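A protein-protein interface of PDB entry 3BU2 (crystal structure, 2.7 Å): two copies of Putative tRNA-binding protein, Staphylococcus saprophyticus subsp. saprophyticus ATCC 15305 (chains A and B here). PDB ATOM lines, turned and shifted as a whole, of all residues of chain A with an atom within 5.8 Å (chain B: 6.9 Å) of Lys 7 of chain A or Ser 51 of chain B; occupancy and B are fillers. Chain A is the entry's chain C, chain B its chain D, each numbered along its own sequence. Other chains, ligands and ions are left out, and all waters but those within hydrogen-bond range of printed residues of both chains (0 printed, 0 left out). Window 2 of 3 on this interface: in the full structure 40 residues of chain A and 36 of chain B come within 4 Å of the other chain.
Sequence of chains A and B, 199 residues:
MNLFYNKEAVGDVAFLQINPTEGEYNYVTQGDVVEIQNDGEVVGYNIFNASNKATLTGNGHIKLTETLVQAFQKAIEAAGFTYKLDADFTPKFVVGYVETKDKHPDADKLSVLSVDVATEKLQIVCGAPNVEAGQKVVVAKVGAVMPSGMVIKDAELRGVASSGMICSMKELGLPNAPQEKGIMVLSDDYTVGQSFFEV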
ATOM      1  N   TYR A   5     -11.987  -8.011   4.384  1.00  0.00           N
ATOM      2  CA  TYR A   5     -11.117  -6.880   4.595  1.00  0.00           C
ATOM      3  C   TYR A   5      -9.671  -7.308   4.784  1.00  0.00           C
ATOM      4  O   TYR A   5      -9.358  -8.096   5.672  1.00  0.00           O
ATOM      5  CB  TYR A   5     -11.578  -6.096   5.824  1.00  0.00           C
ATOM      6  CG  TYR A   5     -10.837  -4.786   6.035  1.00  0.00           C
ATOM      7  CD1 TYR A   5     -11.020  -3.704   5.170  1.00  0.00           C
ATOM      8  CD2 TYR A   5      -9.973  -4.622   7.106  1.00  0.00           C
ATOM      9  CE1 TYR A   5     -10.366  -2.496   5.370  1.00  0.00           C
ATOM     10  CE2 TYR A   5      -9.310  -3.412   7.316  1.00  0.00           C
ATOM     11  CZ  TYR A   5      -9.511  -2.352   6.449  1.00  0.00           C
ATOM     12  OH  TYR A   5      -8.869  -1.147   6.688  1.00  0.00           O
ATOM     13  N   ASN A   6      -8.796  -6.813   3.919  1.00  0.00           N
ATOM     14  CA  ASN A   6      -7.374  -7.071   4.042  1.00  0.00           C
ATOM     15  C   ASN A   6      -6.719  -5.791   3.554  1.00  0.00           C
ATOM     16  O   ASN A   6      -6.375  -5.640   2.379  1.00  0.00           O
ATOM     17  CB  ASN A   6      -6.916  -8.263   3.214  1.00  0.00           C
ATOM     18  CG  ASN A   6      -5.552  -8.802   3.679  1.00  0.00           C
ATOM     19  OD1 ASN A   6      -4.622  -8.036   3.940  1.00  0.00           O
ATOM     20  ND2 ASN A   6      -5.437 -10.118   3.780  1.00  0.00           N
ATOM     21  N   LYS A   7      -6.605  -4.852   4.486  1.00  0.00           N
ATOM     22  CA  LYS A   7      -6.019  -3.544   4.251  1.00  0.00           C
ATOM     23  C   LYS A   7      -4.664  -3.649   3.582  1.00  0.00           C
ATOM     24  O   LYS A   7      -4.398  -2.979   2.580  1.00  0.00           O
ATOM     25  CB  LYS A   7      -5.876  -2.814   5.580  1.00  0.00           C
ATOM     26  CG  LYS A   7      -5.338  -1.407   5.492  1.00  0.00           C
ATOM     27  CD  LYS A   7      -5.354  -0.769   6.887  1.00  0.00           C
ATOM     28  CE  LYS A   7      -4.665   0.591   6.931  1.00  0.00           C
ATOM     29  NZ  LYS A   7      -5.286   1.549   5.972  1.00  0.00           N
ATOM     30  N   GLU A   8      -3.806  -4.500   4.135  1.00  0.00           N
ATOM     31  CA  GLU A   8      -2.472  -4.655   3.588  1.00  0.00           C
ATOM     32  C   GLU A   8      -2.389  -5.447   2.281  1.00  0.00           C
ATOM     33  O   GLU A   8      -1.570  -5.127   1.409  1.00  0.00           O
ATOM     34  CB  GLU A   8      -1.535  -5.245   4.650  1.00  0.00           C
ATOM     35  CG  GLU A   8      -2.202  -6.172   5.676  1.00  0.00           C
ATOM     36  CD  GLU A   8      -2.950  -5.422   6.778  1.00  0.00           C
ATOM     37  OE1 GLU A   8      -2.403  -4.415   7.292  1.00  0.00           O
ATOM     38  OE2 GLU A   8      -4.071  -5.851   7.141  1.00  0.00           O
ATOM     39  N   ALA A   9      -3.247  -6.450   2.114  1.00  0.00           N
ATOM     40  CA  ALA A   9      -3.217  -7.256   0.893  1.00  0.00           C
ATOM     41  C   ALA A   9      -4.082  -6.705  -0.234  1.00  0.00           C
ATOM     42  O   ALA A   9      -3.642  -6.603  -1.373  1.00  0.00           O
ATOM     43  CB  ALA A   9      -3.626  -8.687   1.203  1.00  0.00           C
ATOM     44  N   VAL A  10      -5.319  -6.351   0.086  1.00  0.00           N
ATOM     45  CA  VAL A  10      -6.230  -5.837  -0.924  1.00  0.00           C
ATOM     46  C   VAL A  10      -6.392  -4.327  -0.931  1.00  0.00           C
ATOM     47  O   VAL A  10      -6.354  -3.703  -1.990  1.00  0.00           O
ATOM     48  CB  VAL A  10      -7.587  -6.465  -0.767  1.00  0.00           C
ATOM     49  CG1 VAL A  10      -8.510  -5.964  -1.865  1.00  0.00           C
ATOM     50  CG2 VAL A  10      -7.445  -7.977  -0.808  1.00  0.00           C
ATOM     51  N   GLY A  11      -6.582  -3.742   0.246  1.00  0.00           N
ATOM     52  CA  GLY A  11      -6.731  -2.301   0.327  1.00  0.00           C
ATOM     53  C   GLY A  11      -7.578  -1.864   1.498  1.00  0.00           C
ATOM     54  O   GLY A  11      -8.062  -2.698   2.266  1.00  0.00           O
ATOM     55  N   ASP A  12      -7.756  -0.558   1.658  1.00  0.00           N
ATOM     56  CA  ASP A  12      -8.575  -0.068   2.755  1.00  0.00           C
ATOM     57  C   ASP A  12     -10.004  -0.021   2.259  1.00  0.00           C
ATOM     58  O   ASP A  12     -10.678   1.008   2.351  1.00  0.00           O
ATOM     59  CB  ASP A  12      -8.121   1.322   3.204  1.00  0.00           C
ATOM     60  CG  ASP A  12      -8.594   1.660   4.617  1.00  0.00           C
ATOM     61  OD1 ASP A  12      -8.678   0.729   5.446  1.00  0.00           O
ATOM     62  OD2 ASP A  12      -8.862   2.848   4.907  1.00  0.00           O
ATOM     63  N   VAL A  13     -10.456  -1.150   1.720  1.00  0.00           N
ATOM     64  CA  VAL A  13     -11.807  -1.261   1.188  1.00  0.00           C
ATOM     65  C   VAL A  13     -12.533  -2.442   1.812  1.00  0.00           C
ATOM     66  O   VAL A  13     -12.063  -3.579   1.747  1.00  0.00           O
ATOM     67  CB  VAL A  13     -11.791  -1.465  -0.329  1.00  0.00           C
ATOM     68  CG1 VAL A  13     -13.202  -1.416  -0.863  1.00  0.00           C
ATOM     69  CG2 VAL A  13     -10.923  -0.421  -0.984  1.00  0.00           C
ATOM     70  N   LYS A 109      -3.807   4.559  -4.047  1.00  0.00           N
ATOM     71  CA  LYS A 109      -3.052   3.505  -3.377  1.00  0.00           C
ATOM     72  C   LYS A 109      -3.408   2.132  -3.925  1.00  0.00           C
ATOM     73  O   LYS A 109      -3.092   1.109  -3.319  1.00  0.00           O
ATOM     74  CB  LYS A 109      -3.288   3.546  -1.867  1.00  0.00           C
ATOM     75  CG  LYS A 109      -2.561   4.680  -1.154  1.00  0.00           C
ATOM     76  CD  LYS A 109      -2.915   4.718   0.321  1.00  0.00           C
ATOM     77  CE  LYS A 109      -4.404   5.020   0.509  1.00  0.00           C
ATOM     78  NZ  LYS A 109      -4.826   4.918   1.940  1.00  0.00           N
ATOM     79  N   GLY A 127      -4.308  -3.556  -4.131  1.00  0.00           N
ATOM     80  CA  GLY A 127      -3.678  -2.487  -3.385  1.00  0.00           C
ATOM     81  C   GLY A 127      -2.475  -2.963  -2.588  1.00  0.00           C
ATOM     82  O   GLY A 127      -1.825  -2.171  -1.907  1.00  0.00           O
ATOM     83  N   PRO A 129       0.923  -3.475  -1.316  1.00  0.00           N
ATOM     84  CA  PRO A 129       2.131  -2.693  -1.590  1.00  0.00           C
ATOM     85  C   PRO A 129       3.292  -3.455  -2.205  1.00  0.00           C
ATOM     86  O   PRO A 129       4.119  -2.861  -2.891  1.00  0.00           O
ATOM     87  CB  PRO A 129       2.487  -2.115  -0.222  1.00  0.00           C
ATOM     88  CG  PRO A 129       1.967  -3.135   0.723  1.00  0.00           C
ATOM     89  CD  PRO A 129       0.630  -3.490   0.128  1.00  0.00           C
ATOM     90  N   ILE B  47     -17.110  -0.114   0.684  1.00  0.00           N
ATOM     91  CA  ILE B  47     -16.903   1.164   1.329  1.00  0.00           C
ATOM     92  C   ILE B  47     -15.389   1.342   1.443  1.00  0.00           C
ATOM     93  O   ILE B  47     -14.690   0.498   2.007  1.00  0.00           O
ATOM     94  CB  ILE B  47     -17.654   1.237   2.717  1.00  0.00           C
ATOM     95  CG1 ILE B  47     -16.673   1.130   3.879  1.00  0.00           C
ATOM     96  CG2 ILE B  47     -18.729   0.151   2.804  1.00  0.00           C
ATOM     97  CD1 ILE B  47     -16.001   2.448   4.189  1.00  0.00           C
ATOM     98  N   PHE B  48     -14.891   2.433   0.867  1.00  0.00           N
ATOM     99  CA  PHE B  48     -13.467   2.730   0.861  1.00  0.00           C
ATOM    100  C   PHE B  48     -13.022   3.534   2.070  1.00  0.00           C
ATOM    101  O   PHE B  48     -13.815   4.255   2.670  1.00  0.00           O
ATOM    102  CB  PHE B  48     -13.106   3.442  -0.445  1.00  0.00           C
ATOM    103  CG  PHE B  48     -13.546   2.682  -1.671  1.00  0.00           C
ATOM    104  CD1 PHE B  48     -14.884   2.691  -2.069  1.00  0.00           C
ATOM    105  CD2 PHE B  48     -12.645   1.893  -2.385  1.00  0.00           C
ATOM    106  CE1 PHE B  48     -15.318   1.924  -3.159  1.00  0.00           C
ATOM    107  CE2 PHE B  48     -13.066   1.122  -3.471  1.00  0.00           C
ATOM    108  CZ  PHE B  48     -14.406   1.137  -3.859  1.00  0.00           C
ATOM    109  N   ASN B  49     -11.747   3.405   2.421  1.00  0.00           N
ATOM    110  CA  ASN B  49     -11.197   4.074   3.590  1.00  0.00           C
ATOM    111  C   ASN B  49     -12.006   3.598   4.775  1.00  0.00           C
ATOM    112  O   ASN B  49     -12.270   4.349   5.700  1.00  0.00           O
ATOM    113  CB  ASN B  49     -11.296   5.593   3.473  1.00  0.00           C
ATOM    114  CG  ASN B  49     -10.388   6.155   2.399  1.00  0.00           C
ATOM    115  OD1 ASN B  49      -9.208   5.803   2.315  1.00  0.00           O
ATOM    116  ND2 ASN B  49     -10.930   7.040   1.573  1.00  0.00           N
ATOM    117  N   ALA B  50     -12.399   2.331   4.727  1.00  0.00           N
ATOM    118  CA  ALA B  50     -13.184   1.723   5.784  1.00  0.00           C
ATOM    119  C   ALA B  50     -12.518   1.860   7.147  1.00  0.00           C
ATOM    120  O   ALA B  50     -13.205   1.967   8.167  1.00  0.00           O
ATOM    121  CB  ALA B  50     -13.428   0.258   5.469  1.00  0.00           C
ATOM    122  N   SER B  51     -11.187   1.871   7.171  1.00  0.00           N
ATOM    123  CA  SER B  51     -10.460   1.979   8.431  1.00  0.00           C
ATOM    124  C   SER B  51     -10.796   3.249   9.200  1.00  0.00           C
ATOM    125  O   SER B  51     -10.771   3.249  10.430  1.00  0.00           O
ATOM    126  CB  SER B  51      -8.948   1.911   8.202  1.00  0.00           C
ATOM    127  OG  SER B  51      -8.469   3.054   7.521  1.00  0.00           O
ATOM    128  N   ASN B  52     -11.113   4.330   8.491  1.00  0.00           N
ATOM    129  CA  ASN B  52     -11.450   5.581   9.163  1.00  0.00           C
ATOM    130  C   ASN B  52     -12.968   5.731   9.314  1.00  0.00           C
ATOM    131  O   ASN B  52     -13.473   6.824   9.574  1.00  0.00           O
ATOM    132  CB  ASN B  52     -10.866   6.784   8.401  1.00  0.00           C
ATOM    133  CG  ASN B  52     -11.811   7.329   7.336  1.00  0.00           C
ATOM    134  OD1 ASN B  52     -12.315   6.588   6.493  1.00  0.00           O
ATOM    135  ND2 ASN B  52     -12.051   8.635   7.372  1.00  0.00           N
ATOM    136  N   LYS B  53     -13.686   4.623   9.158  1.00  0.00           N
ATOM    137  CA  LYS B  53     -15.139   4.622   9.286  1.00  0.00           C
ATOM    138  C   LYS B  53     -15.585   3.529  10.250  1.00  0.00           C
ATOM    139  O   LYS B  53     -16.723   3.523  10.720  1.00  0.00           O
ATOM    140  CB  LYS B  53     -15.800   4.398   7.926  1.00  0.00           C
ATOM    141  CG  LYS B  53     -15.536   5.495   6.924  1.00  0.00           C
ATOM    142  CD  LYS B  53     -16.309   5.262   5.634  1.00  0.00           C
ATOM    143  CE  LYS B  53     -15.987   6.327   4.610  1.00  0.00           C
ATOM    144  NZ  LYS B  53     -14.531   6.352   4.308  1.00  0.00           N
ATOM    145  N   ALA B  54     -14.679   2.605  10.542  1.00  0.00           N
ATOM    146  CA  ALA B  54     -14.981   1.516  11.445  1.00  0.00           C
ATOM    147  C   ALA B  54     -13.691   0.920  11.988  1.00  0.00           C
ATOM    148  O   ALA B  54     -12.622   1.070  11.389  1.00  0.00           O
ATOM    149  CB  ALA B  54     -15.780   0.459  10.715  1.00  0.00           C
ATOM    150  N   THR B  55     -13.795   0.246  13.131  1.00  0.00           N
ATOM    151  CA  THR B  55     -12.643  -0.394  13.761  1.00  0.00           C
ATOM    152  C   THR B  55     -12.496  -1.787  13.171  1.00  0.00           C
ATOM    153  O   THR B  55     -13.161  -2.729  13.602  1.00  0.00           O
ATOM    154  CB  THR B  55     -12.833  -0.505  15.274  1.00  0.00           C
ATOM    155  OG1 THR B  55     -13.006   0.805  15.818  1.00  0.00           O
ATOM    156  CG2 THR B  55     -11.624  -1.163  15.914  1.00  0.00           C
ATOM    157  N   LEU B  56     -11.612  -1.900  12.184  1.00  0.00           N
ATOM    158  CA  LEU B  56     -11.379  -3.158  11.496  1.00  0.00           C
ATOM    159  C   LEU B  56     -10.044  -3.812  11.826  1.00  0.00           C
ATOM    160  O   LEU B  56      -9.659  -4.799  11.200  1.00  0.00           O
ATOM    161  CB  LEU B  56     -11.486  -2.930   9.989  1.00  0.00           C
ATOM    162  CG  LEU B  56     -12.871  -2.506   9.503  1.00  0.00           C
ATOM    163  CD1 LEU B  56     -12.779  -1.909   8.113  1.00  0.00           C
ATOM    164  CD2 LEU B  56     -13.803  -3.712   9.526  1.00  0.00           C
ATOM    165  N   THR B  57      -9.334  -3.271  12.809  1.00  0.00           N
ATOM    166  CA  THR B  57      -8.048  -3.840  13.199  1.00  0.00           C
ATOM    167  C   THR B  57      -8.231  -5.074  14.092  1.00  0.00           C
ATOM    168  O   THR B  57      -9.037  -5.962  13.806  1.00  0.00           O
ATOM    169  CB  THR B  57      -7.189  -2.801  13.954  1.00  0.00           C
ATOM    170  OG1 THR B  57      -7.938  -2.265  15.052  1.00  0.00           O
ATOM    171  CG2 THR B  57      -6.780  -1.667  13.028  1.00  0.00           C
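No position is printed for both chains.
Among the printed residues, merely in contact across the chains: Val 13 of chain A with Phe 48 of chain B, Tyr 5 of chain A with Ser 51 of chain B, Asp 12 of chain A with Phe 48 of chain B, Val 13 of chain A with Ile 47 of chain B, Tyr 5 of chain A with Leu 56 of chain B and Lys 7 of chain A with Ser 51 of chain B.
The side-chain amino group of Lys 7 of chain A lies within salt-bridge range of the side-chain carboxylate of Asp 12 of chain A (3.5 Å).
The side-chain amino group (NZ) of Lys 53 of chain B is in hydrogen-bond range of the backbone carbonyl oxygen (O) of Phe 48 of chain B (2.8 Å).
The backbone carbonyl oxygen of Asn 49 of chain B sits at hydrogen-bond distance from the side-chain amino group of Lys 53 of chain B.
The backbone carbonyl oxygen of Asp 12 of chain A is in hydrogen-bond range of the backbone NH of Asn 49 of chain B (2.6 Å).
The backbone carbonyl oxygen of Asp 12 of chain A is in hydrogen-bond range of the backbone NH of Ala 50 of chain B, at 3.2 Å.
OG of Ser 51 of chain B sits at hydrogen-bond distance from OD2 of Asp 12 of chain A (2.7 Å).
Printed residues of chain B that touch a printed residue of chain A: Ile 47, Phe 48, Asn 49, Ala 50, Ser 51 and Leu 56.
Hydrophobic or aromatic side chains of chain A that line the printed part of chain B: Tyr 5 and Val 13.
Among the printed residues, 9 pairs touch across the chains.
Among the printed residues, no Asp or Glu carboxylate lies within 4 Å of a Lys or Arg side-chain nitrogen of the other chain.
Of the printed residues of chain B, Tyr 5 of chain A touches Ser 51 and Leu 56.
Lys 7 of chain A touches just one residue of chain B: Ser 51.
Ala 9 of chain A touches none of the printed residues of chain B.
Of the printed residues of chain B, Asp 12 of chain A touches Phe 48, Asn 49, Ala 50 and Ser 51.
Printed residues of chain A within 4 Å of Ile 47 of chain B: Val 13.
Ser 51 of chain B touches just these residues of chain A: Tyr 5 (3.4 Å), Lys 7 (3.8 Å) and Asp 12 (2.7 Å).
Of the printed residues of chain A, Leu 56 of chain B touches Tyr 5 (3.5 Å).
Thr 57 of chain B touches none of the printed residues of chain A.
The nearest printed residue of chain A that does not touch Ser 51 of chain B is Val 13 of chain A (6.3 Å).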
